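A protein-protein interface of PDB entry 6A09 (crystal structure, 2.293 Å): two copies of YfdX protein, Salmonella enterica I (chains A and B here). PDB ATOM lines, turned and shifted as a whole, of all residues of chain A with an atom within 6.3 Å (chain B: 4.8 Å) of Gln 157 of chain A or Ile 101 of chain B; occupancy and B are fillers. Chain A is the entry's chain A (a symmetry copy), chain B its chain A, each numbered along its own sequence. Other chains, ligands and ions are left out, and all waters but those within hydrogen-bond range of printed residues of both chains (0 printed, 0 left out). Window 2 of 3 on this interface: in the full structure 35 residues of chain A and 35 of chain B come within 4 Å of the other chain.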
ATOM      1  N   ALA A 146      -0.360  17.582  -3.465  1.00  0.00           N
ATOM      2  CA  ALA A 146      -0.324  17.131  -4.853  1.00  0.00           C
ATOM      3  C   ALA A 146      -1.452  17.770  -5.651  1.00  0.00           C
ATOM      4  O   ALA A 146      -1.242  18.232  -6.777  1.00  0.00           O
ATOM      5  CB  ALA A 146      -0.413  15.611  -4.932  1.00  0.00           C
ATOM      6  N   LEU A 149      -0.590  21.317  -6.345  1.00  0.00           N
ATOM      7  CA  LEU A 149       0.394  21.396  -7.418  1.00  0.00           C
ATOM      8  C   LEU A 149      -0.255  21.146  -8.776  1.00  0.00           C
ATOM      9  O   LEU A 149       0.079  21.818  -9.759  1.00  0.00           O
ATOM     10  CB  LEU A 149       1.545  20.412  -7.163  1.00  0.00           C
ATOM     11  CG  LEU A 149       2.446  20.733  -5.959  1.00  0.00           C
ATOM     12  CD1 LEU A 149       3.266  19.522  -5.496  1.00  0.00           C
ATOM     13  CD2 LEU A 149       3.377  21.916  -6.281  1.00  0.00           C
ATOM     14  N   GLY A 153      -0.690  23.749 -12.277  1.00  0.00           N
ATOM     15  CA  GLY A 153      -0.044  23.254 -13.480  1.00  0.00           C
ATOM     16  C   GLY A 153       1.323  22.627 -13.268  1.00  0.00           C
ATOM     17  O   GLY A 153       2.059  22.427 -14.244  1.00  0.00           O
ATOM     18  N   LYS A 154       1.685  22.313 -12.024  1.00  0.00           N
ATOM     19  CA  LYS A 154       3.001  21.752 -11.692  1.00  0.00           C
ATOM     20  C   LYS A 154       2.897  20.226 -11.610  1.00  0.00           C
ATOM     21  O   LYS A 154       2.955  19.608 -10.542  1.00  0.00           O
ATOM     22  CB  LYS A 154       3.520  22.372 -10.394  1.00  0.00           C
ATOM     23  CG  LYS A 154       3.868  23.871 -10.541  1.00  0.00           C
ATOM     24  CD  LYS A 154       3.948  24.599  -9.198  1.00  0.00           C
ATOM     25  CE  LYS A 154       4.190  26.115  -9.342  1.00  0.00           C
ATOM     26  NZ  LYS A 154       4.940  26.520 -10.556  1.00  0.00           N
ATOM     27  N   TYR A 155       2.741  19.621 -12.792  1.00  0.00           N
ATOM     28  CA  TYR A 155       2.315  18.230 -12.863  1.00  0.00           C
ATOM     29  C   TYR A 155       3.440  17.287 -12.446  1.00  0.00           C
ATOM     30  O   TYR A 155       3.228  16.380 -11.630  1.00  0.00           O
ATOM     31  CB  TYR A 155       1.800  17.918 -14.276  1.00  0.00           C
ATOM     32  CG  TYR A 155       0.596  18.775 -14.634  1.00  0.00           C
ATOM     33  CD1 TYR A 155      -0.615  18.620 -13.964  1.00  0.00           C
ATOM     34  CD2 TYR A 155       0.682  19.768 -15.604  1.00  0.00           C
ATOM     35  CE1 TYR A 155      -1.720  19.423 -14.260  1.00  0.00           C
ATOM     36  CE2 TYR A 155      -0.399  20.577 -15.907  1.00  0.00           C
ATOM     37  CZ  TYR A 155      -1.605  20.405 -15.236  1.00  0.00           C
ATOM     38  OH  TYR A 155      -2.695  21.212 -15.549  1.00  0.00           O
ATOM     39  N   TYR A 156       4.647  17.494 -12.983  1.00  0.00           N
ATOM     40  CA  TYR A 156       5.772  16.665 -12.567  1.00  0.00           C
ATOM     41  C   TYR A 156       5.969  16.735 -11.058  1.00  0.00           C
ATOM     42  O   TYR A 156       6.169  15.707 -10.405  1.00  0.00           O
ATOM     43  CB  TYR A 156       7.049  17.077 -13.300  1.00  0.00           C
ATOM     44  CG  TYR A 156       8.195  16.130 -13.022  1.00  0.00           C
ATOM     45  CD1 TYR A 156       8.307  14.933 -13.709  1.00  0.00           C
ATOM     46  CD2 TYR A 156       9.137  16.422 -12.046  1.00  0.00           C
ATOM     47  CE1 TYR A 156       9.344  14.051 -13.448  1.00  0.00           C
ATOM     48  CE2 TYR A 156      10.174  15.555 -11.772  1.00  0.00           C
ATOM     49  CZ  TYR A 156      10.279  14.366 -12.482  1.00  0.00           C
ATOM     50  OH  TYR A 156      11.321  13.498 -12.214  1.00  0.00           O
ATOM     51  N   GLN A 157       5.861  17.936 -10.482  1.00  0.00           N
ATOM     52  CA  GLN A 157       6.006  18.092  -9.038  1.00  0.00           C
ATOM     53  C   GLN A 157       4.892  17.373  -8.276  1.00  0.00           C
ATOM     54  O   GLN A 157       5.138  16.802  -7.204  1.00  0.00           O
ATOM     55  CB  GLN A 157       6.039  19.580  -8.668  1.00  0.00           C
ATOM     56  CG  GLN A 157       7.243  20.336  -9.232  1.00  0.00           C
ATOM     57  CD  GLN A 157       6.952  21.004 -10.581  1.00  0.00           C
ATOM     58  OE1 GLN A 157       6.239  20.454 -11.436  1.00  0.00           O
ATOM     59  NE2 GLN A 157       7.506  22.199 -10.771  1.00  0.00           N
ATOM     60  N   ALA A 158       3.657  17.393  -8.802  1.00  0.00           N
ATOM     61  CA  ALA A 158       2.582  16.630  -8.169  1.00  0.00           C
ATOM     62  C   ALA A 158       2.912  15.142  -8.136  1.00  0.00           C
ATOM     63  O   ALA A 158       2.708  14.471  -7.113  1.00  0.00           O
ATOM     64  CB  ALA A 158       1.255  16.858  -8.901  1.00  0.00           C
ATOM     65  N   GLY A 159       3.399  14.605  -9.266  1.00  0.00           N
ATOM     66  CA  GLY A 159       3.821  13.213  -9.305  1.00  0.00           C
ATOM     67  C   GLY A 159       4.855  12.879  -8.241  1.00  0.00           C
ATOM     68  O   GLY A 159       4.815  11.802  -7.646  1.00  0.00           O
ATOM     69  N   LEU A 160       5.767  13.815  -7.957  1.00  0.00           N
ATOM     70  CA  LEU A 160       6.727  13.607  -6.875  1.00  0.00           C
ATOM     71  C   LEU A 160       6.016  13.360  -5.551  1.00  0.00           C
ATOM     72  O   LEU A 160       6.376  12.447  -4.799  1.00  0.00           O
ATOM     73  CB  LEU A 160       7.677  14.806  -6.760  1.00  0.00           C
ATOM     74  CG  LEU A 160       8.693  14.993  -7.883  1.00  0.00           C
ATOM     75  CD1 LEU A 160       9.612  16.202  -7.603  1.00  0.00           C
ATOM     76  CD2 LEU A 160       9.501  13.739  -8.036  1.00  0.00           C
ATOM     77  N   LEU A 161       4.982  14.133  -5.256  1.00  0.00           N
ATOM     78  CA  LEU A 161       4.318  13.967  -3.967  1.00  0.00           C
ATOM     79  C   LEU A 161       3.475  12.695  -3.934  1.00  0.00           C
ATOM     80  O   LEU A 161       3.392  12.022  -2.898  1.00  0.00           O
ATOM     81  CB  LEU A 161       3.466  15.195  -3.667  1.00  0.00           C
ATOM     82  CG  LEU A 161       4.131  16.264  -2.807  1.00  0.00           C
ATOM     83  CD1 LEU A 161       3.115  17.305  -2.614  1.00  0.00           C
ATOM     84  CD2 LEU A 161       4.568  15.738  -1.438  1.00  0.00           C
ATOM     85  N   LEU A 162       2.832  12.352  -5.049  1.00  0.00           N
ATOM     86  CA  LEU A 162       2.096  11.094  -5.094  1.00  0.00           C
ATOM     87  C   LEU A 162       3.044   9.911  -4.904  1.00  0.00           C
ATOM     88  O   LEU A 162       2.766   9.001  -4.115  1.00  0.00           O
ATOM     89  CB  LEU A 162       1.324  10.990  -6.409  1.00  0.00           C
ATOM     90  CG  LEU A 162       0.219  12.032  -6.640  1.00  0.00           C
ATOM     91  CD1 LEU A 162      -0.420  11.848  -7.989  1.00  0.00           C
ATOM     92  CD2 LEU A 162      -0.850  11.989  -5.556  1.00  0.00           C
ATOM     93  N   LYS B  97      17.112  22.580 -15.098  1.00  0.00           N
ATOM     94  CA  LYS B  97      16.115  21.540 -14.877  1.00  0.00           C
ATOM     95  C   LYS B  97      14.713  22.135 -14.749  1.00  0.00           C
ATOM     96  O   LYS B  97      13.796  21.760 -15.492  1.00  0.00           O
ATOM     97  CB  LYS B  97      16.472  20.720 -13.635  1.00  0.00           C
ATOM     98  CG  LYS B  97      15.301  19.898 -13.129  1.00  0.00           C
ATOM     99  CD  LYS B  97      15.726  18.820 -12.168  1.00  0.00           C
ATOM    100  CE  LYS B  97      14.767  17.647 -12.234  1.00  0.00           C
ATOM    101  NZ  LYS B  97      15.209  16.575 -11.301  1.00  0.00           N
ATOM    102  N   ASN B  98      14.531  23.063 -13.802  1.00  0.00           N
ATOM    103  CA  ASN B  98      13.240  23.725 -13.625  1.00  0.00           C
ATOM    104  C   ASN B  98      12.713  24.299 -14.928  1.00  0.00           C
ATOM    105  O   ASN B  98      11.505  24.279 -15.182  1.00  0.00           O
ATOM    106  CB  ASN B  98      13.354  24.826 -12.577  1.00  0.00           C
ATOM    107  CG  ASN B  98      13.338  24.278 -11.163  1.00  0.00           C
ATOM    108  OD1 ASN B  98      12.276  24.162 -10.543  1.00  0.00           O
ATOM    109  ND2 ASN B  98      14.521  23.914 -10.651  1.00  0.00           N
ATOM    110  N   ASP B  99      13.606  24.794 -15.781  1.00  0.00           N
ATOM    111  CA  ASP B  99      13.164  25.311 -17.070  1.00  0.00           C
ATOM    112  C   ASP B  99      12.554  24.206 -17.924  1.00  0.00           C
ATOM    113  O   ASP B  99      11.462  24.375 -18.486  1.00  0.00           O
ATOM    114  CB  ASP B  99      14.327  26.000 -17.795  1.00  0.00           C
ATOM    115  CG  ASP B  99      14.626  27.396 -17.233  1.00  0.00           C
ATOM    116  OD1 ASP B  99      13.887  27.842 -16.325  1.00  0.00           O
ATOM    117  OD2 ASP B  99      15.588  28.049 -17.698  1.00  0.00           O
ATOM    118  N   ALA B 100      13.228  23.052 -18.013  1.00  0.00           N
ATOM    119  CA  ALA B 100      12.709  21.960 -18.838  1.00  0.00           C
ATOM    120  C   ALA B 100      11.508  21.275 -18.193  1.00  0.00           C
ATOM    121  O   ALA B 100      10.643  20.754 -18.910  1.00  0.00           O
ATOM    122  CB  ALA B 100      13.804  20.931 -19.134  1.00  0.00           C
ATOM    123  N   ILE B 101      11.433  21.260 -16.858  1.00  0.00           N
ATOM    124  CA  ILE B 101      10.249  20.725 -16.186  1.00  0.00           C
ATOM    125  C   ILE B 101       9.014  21.553 -16.545  1.00  0.00           C
ATOM    126  O   ILE B 101       7.949  21.000 -16.851  1.00  0.00           O
ATOM    127  CB  ILE B 101      10.478  20.656 -14.663  1.00  0.00           C
ATOM    128  CG1 ILE B 101      11.479  19.553 -14.311  1.00  0.00           C
ATOM    129  CG2 ILE B 101       9.166  20.386 -13.922  1.00  0.00           C
ATOM    130  CD1 ILE B 101      10.943  18.165 -14.612  1.00  0.00           C
ATOM    131  N   ASN B 102       9.146  22.888 -16.547  1.00  0.00           N
ATOM    132  CA  ASN B 102       8.046  23.758 -16.973  1.00  0.00           C
ATOM    133  C   ASN B 102       7.567  23.398 -18.367  1.00  0.00           C
ATOM    134  O   ASN B 102       6.362  23.327 -18.627  1.00  0.00           O
ATOM    135  CB  ASN B 102       8.481  25.227 -16.939  1.00  0.00           C
ATOM    136  CG  ASN B 102       8.619  25.762 -15.538  1.00  0.00           C
ATOM    137  OD1 ASN B 102       8.036  25.230 -14.596  1.00  0.00           O
ATOM    138  ND2 ASN B 102       9.402  26.817 -15.389  1.00  0.00           N
ATOM    139  N   LYS B 103       8.503  23.157 -19.276  1.00  0.00           N
ATOM    140  CA  LYS B 103       8.153  22.714 -20.617  1.00  0.00           C
ATOM    141  C   LYS B 103       7.439  21.362 -20.583  1.00  0.00           C
ATOM    142  O   LYS B 103       6.426  21.172 -21.270  1.00  0.00           O
ATOM    143  CB  LYS B 103       9.430  22.663 -21.458  1.00  0.00           C
ATOM    144  CG  LYS B 103       9.231  22.430 -22.932  1.00  0.00           C
ATOM    145  CD  LYS B 103      10.488  22.846 -23.674  1.00  0.00           C
ATOM    146  CE  LYS B 103      10.512  22.290 -25.085  1.00  0.00           C
ATOM    147  NZ  LYS B 103       9.361  22.789 -25.885  1.00  0.00           N
ATOM    148  N   ALA B 104       7.941  20.413 -19.774  1.00  0.00           N
ATOM    149  CA  ALA B 104       7.294  19.102 -19.680  1.00  0.00           C
ATOM    150  C   ALA B 104       5.898  19.213 -19.067  1.00  0.00           C
ATOM    151  O   ALA B 104       4.977  18.506 -19.486  1.00  0.00           O
ATOM    152  CB  ALA B 104       8.172  18.130 -18.880  1.00  0.00           C
ATOM    153  N   ASN B 105       5.720  20.116 -18.092  1.00  0.00           N
ATOM    154  CA  ASN B 105       4.391  20.339 -17.522  1.00  0.00           C
ATOM    155  C   ASN B 105       3.412  20.866 -18.567  1.00  0.00           C
ATOM    156  O   ASN B 105       2.233  20.483 -18.574  1.00  0.00           O
ATOM    157  CB  ASN B 105       4.478  21.305 -16.334  1.00  0.00           C
ATOM    158  CG  ASN B 105       5.065  20.652 -15.106  1.00  0.00           C
ATOM    159  OD1 ASN B 105       5.070  19.425 -14.982  1.00  0.00           O
ATOM    160  ND2 ASN B 105       5.556  21.462 -14.183  1.00  0.00           N
ATOM    161  N   LEU B 120      11.159  15.943 -20.719  1.00  0.00           N
ATOM    162  CA  LEU B 120      11.709  15.353 -19.499  1.00  0.00           C
ATOM    163  C   LEU B 120      13.163  14.923 -19.689  1.00  0.00           C
ATOM    164  O   LEU B 120      13.967  15.022 -18.750  1.00  0.00           O
ATOM    165  CB  LEU B 120      10.838  14.181 -19.047  1.00  0.00           C
ATOM    166  CG  LEU B 120       9.511  14.594 -18.409  1.00  0.00           C
ATOM    167  CD1 LEU B 120       8.621  13.368 -18.184  1.00  0.00           C
ATOM    168  CD2 LEU B 120       9.753  15.340 -17.107  1.00  0.00           C
ATOM    169  N   ALA B 123      15.395  17.642 -19.050  1.00  0.00           N
ATOM    170  CA  ALA B 123      15.473  17.858 -17.611  1.00  0.00           C
ATOM    171  C   ALA B 123      16.278  16.779 -16.913  1.00  0.00           C
ATOM    172  O   ALA B 123      16.312  16.744 -15.679  1.00  0.00           O
ATOM    173  CB  ALA B 123      14.064  17.936 -17.012  1.00  0.00           C
ATOM    174  N   VAL B 125      15.613  13.575 -16.974  1.00  0.00           N
ATOM    175  CA  VAL B 125      14.674  12.617 -16.407  1.00  0.00           C
ATOM    176  C   VAL B 125      14.395  11.523 -17.429  1.00  0.00           C
ATOM    177  O   VAL B 125      13.898  11.795 -18.529  1.00  0.00           O
ATOM    178  CB  VAL B 125      13.371  13.298 -15.963  1.00  0.00           C
ATOM    179  CG1 VAL B 125      12.374  12.231 -15.503  1.00  0.00           C
ATOM    180  CG2 VAL B 125      13.657  14.316 -14.850  1.00  0.00           C
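Printed residues of chain B that touch a printed residue of chain A: Ile 101, Asn 105, Leu 120 and Val 125. Among the printed residues, 9 pairs touch across the chains. Among the printed residues, no Asp or Glu carboxylate lies within 4 Å of a Lys or Arg side-chain nitrogen of the other chain.
The backbone carbonyl oxygen (O) of Leu 149 of chain A sits at hydrogen-bond distance from the backbone NH (N) of Lys 154 of chain A (2.8 Å). The backbone carbonyl oxygen (O) of Leu 120 of chain B sits at hydrogen-bond distance from the backbone NH (N) of Val 125 of chain B.
The side-chain amide oxygen (OE1) of Gln 157 of chain A is in hydrogen-bond range of the side-chain amide nitrogen (ND2) of Asn 105 of chain B, at 3.0 Å. The side-chain amide oxygen (OD1) of Asn 105 of chain B sits at hydrogen-bond distance from the backbone NH (N) of Tyr 156 of chain A (2.8 Å). The side-chain amide oxygen of Asn 105 of chain B is in hydrogen-bond range of the backbone NH of Tyr 155 of chain A, 3.2 Å away.
Among the printed residues, pairs that only touch across the chains: Gly 153 of chain A with Asn 105 of chain B (3.4 Å), Lys 154 of chain A with Asn 105 of chain B (3.6 Å), Tyr 156 of chain A with Ile 101 of chain B (3.6 Å), Tyr 156 of chain A with Leu 120 of chain B (3.7 Å), Tyr 156 of chain A with Val 125 of chain B (3.6 Å) and Gln 157 of chain A with Ile 101 of chain B (3.8 Å).
Of chain B, only Ile 101 (3.8 Å) and Asn 105 (3.0 Å) come within 4 Å of Gln 157 of chain A. Ile 101 of chain B touches just these residues of chain A: Tyr 156 (3.6 Å) and Gln 157 (3.8 Å). Of the printed residues of chain A, Asn 105 of chain B touches Gly 153 (3.4 Å), Lys 154 (3.6 Å), Tyr 155 (3.2 Å), Tyr 156 (2.8 Å) and Gln 157 (3.0 Å). Printed residues of chain B within 4 Å of Tyr 155 of chain A: Asn 105 (3.2 Å). Asp 99 of chain B touches none of the printed residues of chain A. The nearest printed residue of chain B that does not touch Gln 157 of chain A is Asn 102 of chain B (4.9 Å).
No position is printed for both chains. Of the 9 pairs that touch across the chains among the printed residues, none has its exchanged pair printed and touching as well.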
